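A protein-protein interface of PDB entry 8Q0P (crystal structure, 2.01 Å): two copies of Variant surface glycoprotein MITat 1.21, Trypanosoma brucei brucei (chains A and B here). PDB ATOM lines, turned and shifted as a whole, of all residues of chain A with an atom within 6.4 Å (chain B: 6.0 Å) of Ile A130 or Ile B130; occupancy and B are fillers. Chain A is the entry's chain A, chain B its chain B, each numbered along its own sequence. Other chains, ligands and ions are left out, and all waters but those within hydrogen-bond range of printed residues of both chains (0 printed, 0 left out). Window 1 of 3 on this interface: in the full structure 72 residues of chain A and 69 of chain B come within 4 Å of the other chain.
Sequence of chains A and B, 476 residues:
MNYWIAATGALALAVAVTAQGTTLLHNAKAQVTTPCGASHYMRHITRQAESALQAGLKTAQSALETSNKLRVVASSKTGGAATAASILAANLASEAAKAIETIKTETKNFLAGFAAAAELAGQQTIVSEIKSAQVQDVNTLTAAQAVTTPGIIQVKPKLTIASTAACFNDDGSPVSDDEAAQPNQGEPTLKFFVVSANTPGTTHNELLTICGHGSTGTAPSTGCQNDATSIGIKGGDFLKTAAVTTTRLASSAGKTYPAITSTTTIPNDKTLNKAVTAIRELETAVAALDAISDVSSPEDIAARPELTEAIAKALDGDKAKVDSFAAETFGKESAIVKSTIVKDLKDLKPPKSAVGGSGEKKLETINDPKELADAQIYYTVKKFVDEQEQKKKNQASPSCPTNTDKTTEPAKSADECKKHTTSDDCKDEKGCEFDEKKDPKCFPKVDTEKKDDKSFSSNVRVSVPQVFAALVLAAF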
ATOM      1  N   THR A 125      -5.035  20.598 -21.983  1.00  0.00           N
ATOM      2  CA  THR A 125      -6.079  21.571 -22.269  1.00  0.00           C
ATOM      3  C   THR A 125      -7.393  21.184 -21.598  1.00  0.00           C
ATOM      4  O   THR A 125      -8.098  22.043 -21.052  1.00  0.00           O
ATOM      5  CB  THR A 125      -6.264  21.699 -23.780  1.00  0.00           C
ATOM      6  OG1 THR A 125      -5.055  22.192 -24.365  1.00  0.00           O
ATOM      7  CG2 THR A 125      -7.396  22.659 -24.093  1.00  0.00           C
ATOM      8  N   ILE A 126      -7.739  19.895 -21.628  1.00  0.00           N
ATOM      9  CA  ILE A 126      -8.935  19.452 -20.921  1.00  0.00           C
ATOM     10  C   ILE A 126      -8.740  19.552 -19.417  1.00  0.00           C
ATOM     11  O   ILE A 126      -9.667  19.933 -18.691  1.00  0.00           O
ATOM     12  CB  ILE A 126      -9.332  18.027 -21.338  1.00  0.00           C
ATOM     13  CG1 ILE A 126      -9.466  17.945 -22.860  1.00  0.00           C
ATOM     14  CG2 ILE A 126     -10.680  17.672 -20.712  1.00  0.00           C
ATOM     15  CD1 ILE A 126     -10.685  18.697 -23.384  1.00  0.00           C
ATOM     16  N   VAL A 127      -7.543  19.210 -18.923  1.00  0.00           N
ATOM     17  CA  VAL A 127      -7.269  19.354 -17.494  1.00  0.00           C
ATOM     18  C   VAL A 127      -7.479  20.798 -17.066  1.00  0.00           C
ATOM     19  O   VAL A 127      -8.042  21.065 -16.002  1.00  0.00           O
ATOM     20  CB  VAL A 127      -5.847  18.853 -17.155  1.00  0.00           C
ATOM     21  CG1 VAL A 127      -5.393  19.358 -15.767  1.00  0.00           C
ATOM     22  CG2 VAL A 127      -5.781  17.332 -17.212  1.00  0.00           C
ATOM     23  N   SER A 128      -7.073  21.754 -17.904  1.00  0.00           N
ATOM     24  CA  SER A 128      -7.211  23.156 -17.515  1.00  0.00           C
ATOM     25  C   SER A 128      -8.680  23.586 -17.437  1.00  0.00           C
ATOM     26  O   SER A 128      -9.020  24.501 -16.682  1.00  0.00           O
ATOM     27  CB  SER A 128      -6.439  24.046 -18.489  1.00  0.00           C
ATOM     28  OG  SER A 128      -7.193  24.310 -19.667  1.00  0.00           O
ATOM     29  N   GLU A 129      -9.566  22.945 -18.198  1.00  0.00           N
ATOM     30  CA  GLU A 129     -10.976  23.286 -18.132  1.00  0.00           C
ATOM     31  C   GLU A 129     -11.692  22.553 -17.007  1.00  0.00           C
ATOM     32  O   GLU A 129     -12.488  23.158 -16.285  1.00  0.00           O
ATOM     33  CB  GLU A 129     -11.647  22.982 -19.479  1.00  0.00           C
ATOM     34  CG  GLU A 129     -11.287  23.990 -20.566  1.00  0.00           C
ATOM     35  CD  GLU A 129     -11.929  25.362 -20.300  1.00  0.00           C
ATOM     36  OE1 GLU A 129     -11.248  26.226 -19.679  1.00  0.00           O
ATOM     37  OE2 GLU A 129     -13.110  25.576 -20.699  1.00  0.00           O
ATOM     38  N   ILE A 130     -11.424  21.263 -16.827  1.00  0.00           N
ATOM     39  CA  ILE A 130     -12.180  20.435 -15.843  1.00  0.00           C
ATOM     40  C   ILE A 130     -11.802  20.751 -14.385  1.00  0.00           C
ATOM     41  O   ILE A 130     -12.619  20.484 -13.511  1.00  0.00           O
ATOM     42  CB  ILE A 130     -12.003  18.942 -16.175  1.00  0.00           C
ATOM     43  CG1 ILE A 130     -13.127  18.089 -15.584  1.00  0.00           C
ATOM     44  CG2 ILE A 130     -10.632  18.440 -15.754  1.00  0.00           C
ATOM     45  CD1 ILE A 130     -14.508  18.530 -15.995  1.00  0.00           C
ATOM     46  N   LYS A 131     -10.612  21.297 -14.141  1.00  0.00           N
ATOM     47  CA  LYS A 131     -10.162  21.600 -12.756  1.00  0.00           C
ATOM     48  C   LYS A 131     -11.151  22.565 -12.094  1.00  0.00           C
ATOM     49  O   LYS A 131     -11.213  22.574 -10.868  1.00  0.00           O
ATOM     50  CB  LYS A 131      -8.744  22.180 -12.748  1.00  0.00           C
ATOM     51  CG  LYS A 131      -8.571  23.502 -13.477  1.00  0.00           C
ATOM     52  CD  LYS A 131      -7.130  23.929 -13.585  1.00  0.00           C
ATOM     53  CE  LYS A 131      -6.767  25.013 -12.595  1.00  0.00           C
ATOM     54  NZ  LYS A 131      -6.341  24.449 -11.294  1.00  0.00           N
ATOM     55  N   SER A 132     -11.891  23.327 -12.891  1.00  0.00           N
ATOM     56  CA  SER A 132     -12.876  24.314 -12.385  1.00  0.00           C
ATOM     57  C   SER A 132     -14.140  23.641 -11.845  1.00  0.00           C
ATOM     58  O   SER A 132     -14.979  24.358 -11.305  1.00  0.00           O
ATOM     59  CB  SER A 132     -13.230  25.249 -13.504  1.00  0.00           C
ATOM     60  OG  SER A 132     -14.141  24.639 -14.408  1.00  0.00           O
ATOM     61  N   ALA A 133     -14.275  22.324 -11.984  1.00  0.00           N
ATOM     62  CA  ALA A 133     -15.532  21.691 -11.598  1.00  0.00           C
ATOM     63  C   ALA A 133     -15.820  21.886 -10.114  1.00  0.00           C
ATOM     64  O   ALA A 133     -14.958  21.648  -9.259  1.00  0.00           O
ATOM     65  CB  ALA A 133     -15.498  20.202 -11.928  1.00  0.00           C
ATOM     66  N   GLN A 134     -17.051  22.300  -9.808  1.00  0.00           N
ATOM     67  CA  GLN A 134     -17.434  22.591  -8.435  1.00  0.00           C
ATOM     68  C   GLN A 134     -18.834  22.074  -8.146  1.00  0.00           C
ATOM     69  O   GLN A 134     -19.661  21.939  -9.048  1.00  0.00           O
ATOM     70  CB  GLN A 134     -17.385  24.098  -8.154  1.00  0.00           C
ATOM     71  CG  GLN A 134     -15.960  24.627  -8.055  1.00  0.00           C
ATOM     72  CD  GLN A 134     -15.893  26.023  -7.479  1.00  0.00           C
ATOM     73  OE1 GLN A 134     -16.588  26.929  -7.943  1.00  0.00           O
ATOM     74  NE2 GLN A 134     -15.056  26.207  -6.461  1.00  0.00           N
ATOM     75  N   LEU A 159     -19.545  23.915 -13.990  1.00  0.00           N
ATOM     76  CA  LEU A 159     -18.271  24.076 -14.666  1.00  0.00           C
ATOM     77  C   LEU A 159     -18.094  25.541 -15.032  1.00  0.00           C
ATOM     78  O   LEU A 159     -19.059  26.302 -15.126  1.00  0.00           O
ATOM     79  CB  LEU A 159     -18.192  23.205 -15.933  1.00  0.00           C
ATOM     80  CG  LEU A 159     -18.402  21.695 -15.769  1.00  0.00           C
ATOM     81  CD1 LEU A 159     -18.676  21.003 -17.123  1.00  0.00           C
ATOM     82  CD2 LEU A 159     -17.202  21.073 -15.083  1.00  0.00           C
ATOM     83  N   THR A 160     -16.843  25.933 -15.212  1.00  0.00           N
ATOM     84  CA  THR A 160     -16.474  27.253 -15.710  1.00  0.00           C
ATOM     85  C   THR A 160     -15.871  27.052 -17.095  1.00  0.00           C
ATOM     86  O   THR A 160     -14.758  26.524 -17.222  1.00  0.00           O
ATOM     87  CB  THR A 160     -15.480  27.941 -14.772  1.00  0.00           C
ATOM     88  OG1 THR A 160     -16.075  28.099 -13.477  1.00  0.00           O
ATOM     89  CG2 THR A 160     -15.088  29.311 -15.313  1.00  0.00           C
ATOM     90  N   VAL A 195      -5.578  15.358 -12.300  1.00  0.00           N
ATOM     91  CA  VAL A 195      -6.693  15.567 -11.376  1.00  0.00           C
ATOM     92  C   VAL A 195      -7.084  14.259 -10.695  1.00  0.00           C
ATOM     93  O   VAL A 195      -6.848  13.158 -11.203  1.00  0.00           O
ATOM     94  CB  VAL A 195      -7.926  16.210 -12.059  1.00  0.00           C
ATOM     95  CG1 VAL A 195      -7.569  17.572 -12.620  1.00  0.00           C
ATOM     96  CG2 VAL A 195      -8.509  15.304 -13.145  1.00  0.00           C
ATOM     97  N   LEU A 239     -12.672  18.419  -7.831  1.00  0.00           N
ATOM     98  CA  LEU A 239     -11.400  17.765  -8.096  1.00  0.00           C
ATOM     99  C   LEU A 239     -10.264  18.411  -7.318  1.00  0.00           C
ATOM    100  O   LEU A 239     -10.327  19.574  -6.910  1.00  0.00           O
ATOM    101  CB  LEU A 239     -11.050  17.797  -9.587  1.00  0.00           C
ATOM    102  CG  LEU A 239     -12.076  17.155 -10.519  1.00  0.00           C
ATOM    103  CD1 LEU A 239     -11.804  17.560 -11.963  1.00  0.00           C
ATOM    104  CD2 LEU A 239     -12.062  15.642 -10.374  1.00  0.00           C
ATOM    105  N   ILE A 266      -6.056  11.450 -13.353  1.00  0.00           N
ATOM    106  CA  ILE A 266      -6.415  11.615 -14.753  1.00  0.00           C
ATOM    107  C   ILE A 266      -5.607  12.786 -15.297  1.00  0.00           C
ATOM    108  O   ILE A 266      -5.750  13.910 -14.809  1.00  0.00           O
ATOM    109  CB  ILE A 266      -7.920  11.869 -14.951  1.00  0.00           C
ATOM    110  CG1 ILE A 266      -8.748  10.710 -14.397  1.00  0.00           C
ATOM    111  CG2 ILE A 266      -8.209  12.099 -16.426  1.00  0.00           C
ATOM    112  CD1 ILE A 266     -10.291  11.010 -14.359  1.00  0.00           C
ATOM    113  N   THR B 125      -9.149  11.330 -24.954  1.00  0.00           N
ATOM    114  CA  THR B 125      -8.667  10.395 -23.944  1.00  0.00           C
ATOM    115  C   THR B 125      -9.041  10.858 -22.536  1.00  0.00           C
ATOM    116  O   THR B 125      -9.429  10.042 -21.693  1.00  0.00           O
ATOM    117  CB  THR B 125      -7.152  10.221 -24.072  1.00  0.00           C
ATOM    118  OG1 THR B 125      -6.845   9.648 -25.350  1.00  0.00           O
ATOM    119  CG2 THR B 125      -6.628   9.292 -22.989  1.00  0.00           C
ATOM    120  N   ILE B 126      -8.922  12.155 -22.251  1.00  0.00           N
ATOM    121  CA  ILE B 126      -9.299  12.629 -20.921  1.00  0.00           C
ATOM    122  C   ILE B 126     -10.817  12.618 -20.768  1.00  0.00           C
ATOM    123  O   ILE B 126     -11.342  12.230 -19.717  1.00  0.00           O
ATOM    124  CB  ILE B 126      -8.718  14.025 -20.639  1.00  0.00           C
ATOM    125  CG1 ILE B 126      -7.190  14.035 -20.783  1.00  0.00           C
ATOM    126  CG2 ILE B 126      -9.104  14.477 -19.217  1.00  0.00           C
ATOM    127  CD1 ILE B 126      -6.462  13.105 -19.802  1.00  0.00           C
ATOM    128  N   VAL B 127     -11.548  13.025 -21.815  1.00  0.00           N
ATOM    129  CA  VAL B 127     -13.009  12.944 -21.773  1.00  0.00           C
ATOM    130  C   VAL B 127     -13.449  11.533 -21.398  1.00  0.00           C
ATOM    131  O   VAL B 127     -14.334  11.349 -20.551  1.00  0.00           O
ATOM    132  CB  VAL B 127     -13.618  13.397 -23.117  1.00  0.00           C
ATOM    133  CG1 VAL B 127     -15.068  12.955 -23.219  1.00  0.00           C
ATOM    134  CG2 VAL B 127     -13.509  14.909 -23.271  1.00  0.00           C
ATOM    135  N   SER B 128     -12.808  10.511 -21.985  1.00  0.00           N
ATOM    136  CA  SER B 128     -13.181   9.131 -21.681  1.00  0.00           C
ATOM    137  C   SER B 128     -12.932   8.757 -20.225  1.00  0.00           C
ATOM    138  O   SER B 128     -13.586   7.841 -19.719  1.00  0.00           O
ATOM    139  CB  SER B 128     -12.430   8.151 -22.583  1.00  0.00           C
ATOM    140  OG  SER B 128     -11.240   7.672 -21.966  1.00  0.00           O
ATOM    141  N   GLU B 129     -11.994   9.424 -19.545  1.00  0.00           N
ATOM    142  CA  GLU B 129     -11.733   9.141 -18.138  1.00  0.00           C
ATOM    143  C   GLU B 129     -12.644   9.942 -17.212  1.00  0.00           C
ATOM    144  O   GLU B 129     -13.192   9.395 -16.253  1.00  0.00           O
ATOM    145  CB  GLU B 129     -10.263   9.454 -17.795  1.00  0.00           C
ATOM    146  CG  GLU B 129      -9.225   8.397 -18.238  1.00  0.00           C
ATOM    147  CD  GLU B 129      -9.410   7.057 -17.533  1.00  0.00           C
ATOM    148  OE1 GLU B 129     -10.256   6.250 -17.991  1.00  0.00           O
ATOM    149  OE2 GLU B 129      -8.736   6.831 -16.492  1.00  0.00           O
ATOM    150  N   ILE B 130     -12.788  11.248 -17.455  1.00  0.00           N
ATOM    151  CA  ILE B 130     -13.560  12.078 -16.535  1.00  0.00           C
ATOM    152  C   ILE B 130     -15.065  11.836 -16.657  1.00  0.00           C
ATOM    153  O   ILE B 130     -15.811  12.123 -15.714  1.00  0.00           O
ATOM    154  CB  ILE B 130     -13.248  13.572 -16.751  1.00  0.00           C
ATOM    155  CG1 ILE B 130     -13.741  14.024 -18.127  1.00  0.00           C
ATOM    156  CG2 ILE B 130     -11.748  13.830 -16.627  1.00  0.00           C
ATOM    157  CD1 ILE B 130     -13.600  15.518 -18.380  1.00  0.00           C
ATOM    158  N   LYS B 131     -15.540  11.306 -17.787  1.00  0.00           N
ATOM    159  CA  LYS B 131     -16.967  11.043 -17.904  1.00  0.00           C
ATOM    160  C   LYS B 131     -17.467  10.084 -16.827  1.00  0.00           C
ATOM    161  O   LYS B 131     -18.683   9.950 -16.656  1.00  0.00           O
ATOM    162  CB  LYS B 131     -17.290  10.499 -19.301  1.00  0.00           C
ATOM    163  CG  LYS B 131     -16.947   9.028 -19.501  1.00  0.00           C
ATOM    164  CD  LYS B 131     -17.405   8.529 -20.865  1.00  0.00           C
ATOM    165  CE  LYS B 131     -17.591   7.015 -20.862  1.00  0.00           C
ATOM    166  NZ  LYS B 131     -18.196   6.515 -22.133  1.00  0.00           N
ATOM    167  N   SER B 132     -16.562   9.435 -16.087  1.00  0.00           N
ATOM    168  CA  SER B 132     -16.923   8.547 -14.989  1.00  0.00           C
ATOM    169  C   SER B 132     -17.242   9.291 -13.694  1.00  0.00           C
ATOM    170  O   SER B 132     -17.608   8.645 -12.707  1.00  0.00           O
ATOM    171  CB  SER B 132     -15.779   7.565 -14.722  1.00  0.00           C
ATOM    172  OG  SER B 132     -14.753   8.189 -13.932  1.00  0.00           O
ATOM    173  N   ALA B 133     -17.075  10.610 -13.664  1.00  0.00           N
ATOM    174  CA  ALA B 133     -17.186  11.361 -12.419  1.00  0.00           C
ATOM    175  C   ALA B 133     -18.591  11.246 -11.840  1.00  0.00           C
ATOM    176  O   ALA B 133     -19.589  11.431 -12.545  1.00  0.00           O
ATOM    177  CB  ALA B 133     -16.845  12.830 -12.663  1.00  0.00           C
ATOM    178  N   LEU B 159     -14.139   9.112  -8.950  1.00  0.00           N
ATOM    179  CA  LEU B 159     -13.711   8.863 -10.312  1.00  0.00           C
ATOM    180  C   LEU B 159     -13.434   7.374 -10.474  1.00  0.00           C
ATOM    181  O   LEU B 159     -13.234   6.647  -9.498  1.00  0.00           O
ATOM    182  CB  LEU B 159     -12.452   9.674 -10.662  1.00  0.00           C
ATOM    183  CG  LEU B 159     -12.579  11.198 -10.685  1.00  0.00           C
ATOM    184  CD1 LEU B 159     -11.195  11.870 -10.727  1.00  0.00           C
ATOM    185  CD2 LEU B 159     -13.430  11.624 -11.865  1.00  0.00           C
ATOM    186  N   VAL B 195     -18.276  17.069 -22.496  1.00  0.00           N
ATOM    187  CA  VAL B 195     -18.951  16.939 -21.209  1.00  0.00           C
ATOM    188  C   VAL B 195     -19.518  18.288 -20.785  1.00  0.00           C
ATOM    189  O   VAL B 195     -19.029  19.353 -21.179  1.00  0.00           O
ATOM    190  CB  VAL B 195     -18.018  16.366 -20.116  1.00  0.00           C
ATOM    191  CG1 VAL B 195     -17.342  15.073 -20.614  1.00  0.00           C
ATOM    192  CG2 VAL B 195     -16.970  17.388 -19.691  1.00  0.00           C
ATOM    193  N   PHE B 238     -21.772  13.289 -12.215  1.00  0.00           N
ATOM    194  CA  PHE B 238     -21.483  14.713 -12.104  1.00  0.00           C
ATOM    195  C   PHE B 238     -21.613  15.418 -13.449  1.00  0.00           C
ATOM    196  O   PHE B 238     -21.942  16.609 -13.496  1.00  0.00           O
ATOM    197  CB  PHE B 238     -20.076  14.899 -11.526  1.00  0.00           C
ATOM    198  CG  PHE B 238     -19.710  16.332 -11.256  1.00  0.00           C
ATOM    199  CD1 PHE B 238     -20.007  16.915 -10.038  1.00  0.00           C
ATOM    200  CD2 PHE B 238     -19.075  17.095 -12.223  1.00  0.00           C
ATOM    201  CE1 PHE B 238     -19.676  18.233  -9.785  1.00  0.00           C
ATOM    202  CE2 PHE B 238     -18.737  18.415 -11.976  1.00  0.00           C
ATOM    203  CZ  PHE B 238     -19.042  18.986 -10.748  1.00  0.00           C
ATOM    204  N   LEU B 239     -21.357  14.703 -14.543  1.00  0.00           N
ATOM    205  CA  LEU B 239     -21.338  15.250 -15.889  1.00  0.00           C
ATOM    206  C   LEU B 239     -22.337  14.505 -16.767  1.00  0.00           C
ATOM    207  O   LEU B 239     -22.691  13.355 -16.503  1.00  0.00           O
ATOM    208  CB  LEU B 239     -19.941  15.135 -16.529  1.00  0.00           C
ATOM    209  CG  LEU B 239     -18.736  15.664 -15.764  1.00  0.00           C
ATOM    210  CD1 LEU B 239     -17.435  15.171 -16.408  1.00  0.00           C
ATOM    211  CD2 LEU B 239     -18.774  17.198 -15.699  1.00  0.00           C
ATOM    212  N   ILE B 266     -16.965  20.924 -22.386  1.00  0.00           N
ATOM    213  CA  ILE B 266     -15.524  20.718 -22.392  1.00  0.00           C
ATOM    214  C   ILE B 266     -15.216  19.506 -23.269  1.00  0.00           C
ATOM    215  O   ILE B 266     -15.638  18.389 -22.952  1.00  0.00           O
ATOM    216  CB  ILE B 266     -14.974  20.511 -20.971  1.00  0.00           C
ATOM    217  CG1 ILE B 266     -15.278  21.733 -20.098  1.00  0.00           C
ATOM    218  CG2 ILE B 266     -13.485  20.212 -21.019  1.00  0.00           C
ATOM    219  CD1 ILE B 266     -14.917  21.530 -18.616  1.00  0.00           C
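The backbone carbonyl oxygen (O) of Val B195 lies within hydrogen-bond range of the backbone NH (N) of Ile B266 (2.9 Å). O of Val A195 sits at hydrogen-bond distance from N of Ile A266 (2.9 Å). The backbone carbonyl oxygen (O) of Glu B129 is in hydrogen-bond range of the side-chain hydroxyl (OG) of Ser B132, at 3.0 Å. The backbone carbonyl oxygen (O) of Ala B133 sits at hydrogen-bond distance from the backbone NH (N) of Phe B238 (2.9 Å). The side-chain hydroxyl (OG) of Ser A132 sits at hydrogen-bond distance from the backbone carbonyl oxygen (O) of Glu A129 (2.9 Å).
Among the printed residues, merely in contact across the chains: Ile A126 with Ile B126, Ile A126 with Ile B266, Glu A129 with Ile B266, Ile A130 with Ile B130, Ile A130 with Ile B266, Ala A133 with Phe B238, Gln A134 with Phe B238, Leu A239 with Leu B159, Ile A266 with Ile B126, Ile A266 with Glu B129, Ile A266 with Ile B130 and Ile A266 with Leu B159.
Of chain A, only Ile A130 (3.8 Å) and Ile A266 (3.9 Å) come within 4 Å of Ile B130. Printed residues of chain A within 4 Å of Phe B238: Ala A133 (3.7 Å) and Gln A134 (3.5 Å). Printed residues of chain B within 4 Å of Ile A266: Ile B126, Glu B129, Ile B130 and Leu B159. Printed residues of chain A within 4 Å of Leu B159: Leu A239 (3.9 Å) and Ile A266 (3.8 Å). Of the printed residues of chain A, Glu B129 touches Ile A266. Printed residues of chain A within 4 Å of Ile B126: Ile A126 (3.9 Å) and Ile A266 (3.8 Å). Leu A159 touches none of the printed residues of chain B. The nearest residue of chain B that does not touch Ile A130 is Leu B239 (4.5 Å).
Hydrophobic or aromatic side chains of chain A within 4 Å of the printed part of chain B: Ile A126, Ile A130, Ala A133, Leu A239 and Ile A266. Along chain A the printed residues that touch a printed residue of chain B span positions 126 to 266. Printed residues of chain B that touch a printed residue of chain A: Ile B126, Glu B129, Ile B130, Leu B159, Phe B238 and Ile B266. Hydrophobic or aromatic side chains of chain B that line the printed part of chain A: Ile B126, Ile B130, Leu B159, Phe B238 and Ile B266. Among the printed residues, 12 pairs touch across the chains. Among the printed residues, no Asp or Glu carboxylate lies within 4 Å of a Lys or Arg side-chain nitrogen of the other chain.
Ile A126 touches its own counterpart, Ile B126. Glu A129 touches Ile B266, and with the chains exchanged Ile A266 touches Glu B129. Ile A130 touches its own counterpart, Ile B130. Ile A130 touches Ile B266, and with the chains exchanged Ile A266 touches Ile B130. Positions printed for both chains: 125, 126, 127, 128, 129, 130, 131, 132, 133, 159, 195, 239 and 266. Of the 12 pairs that touch across the chains among the printed residues, 8 have their exchanged pair printed and touching as well.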
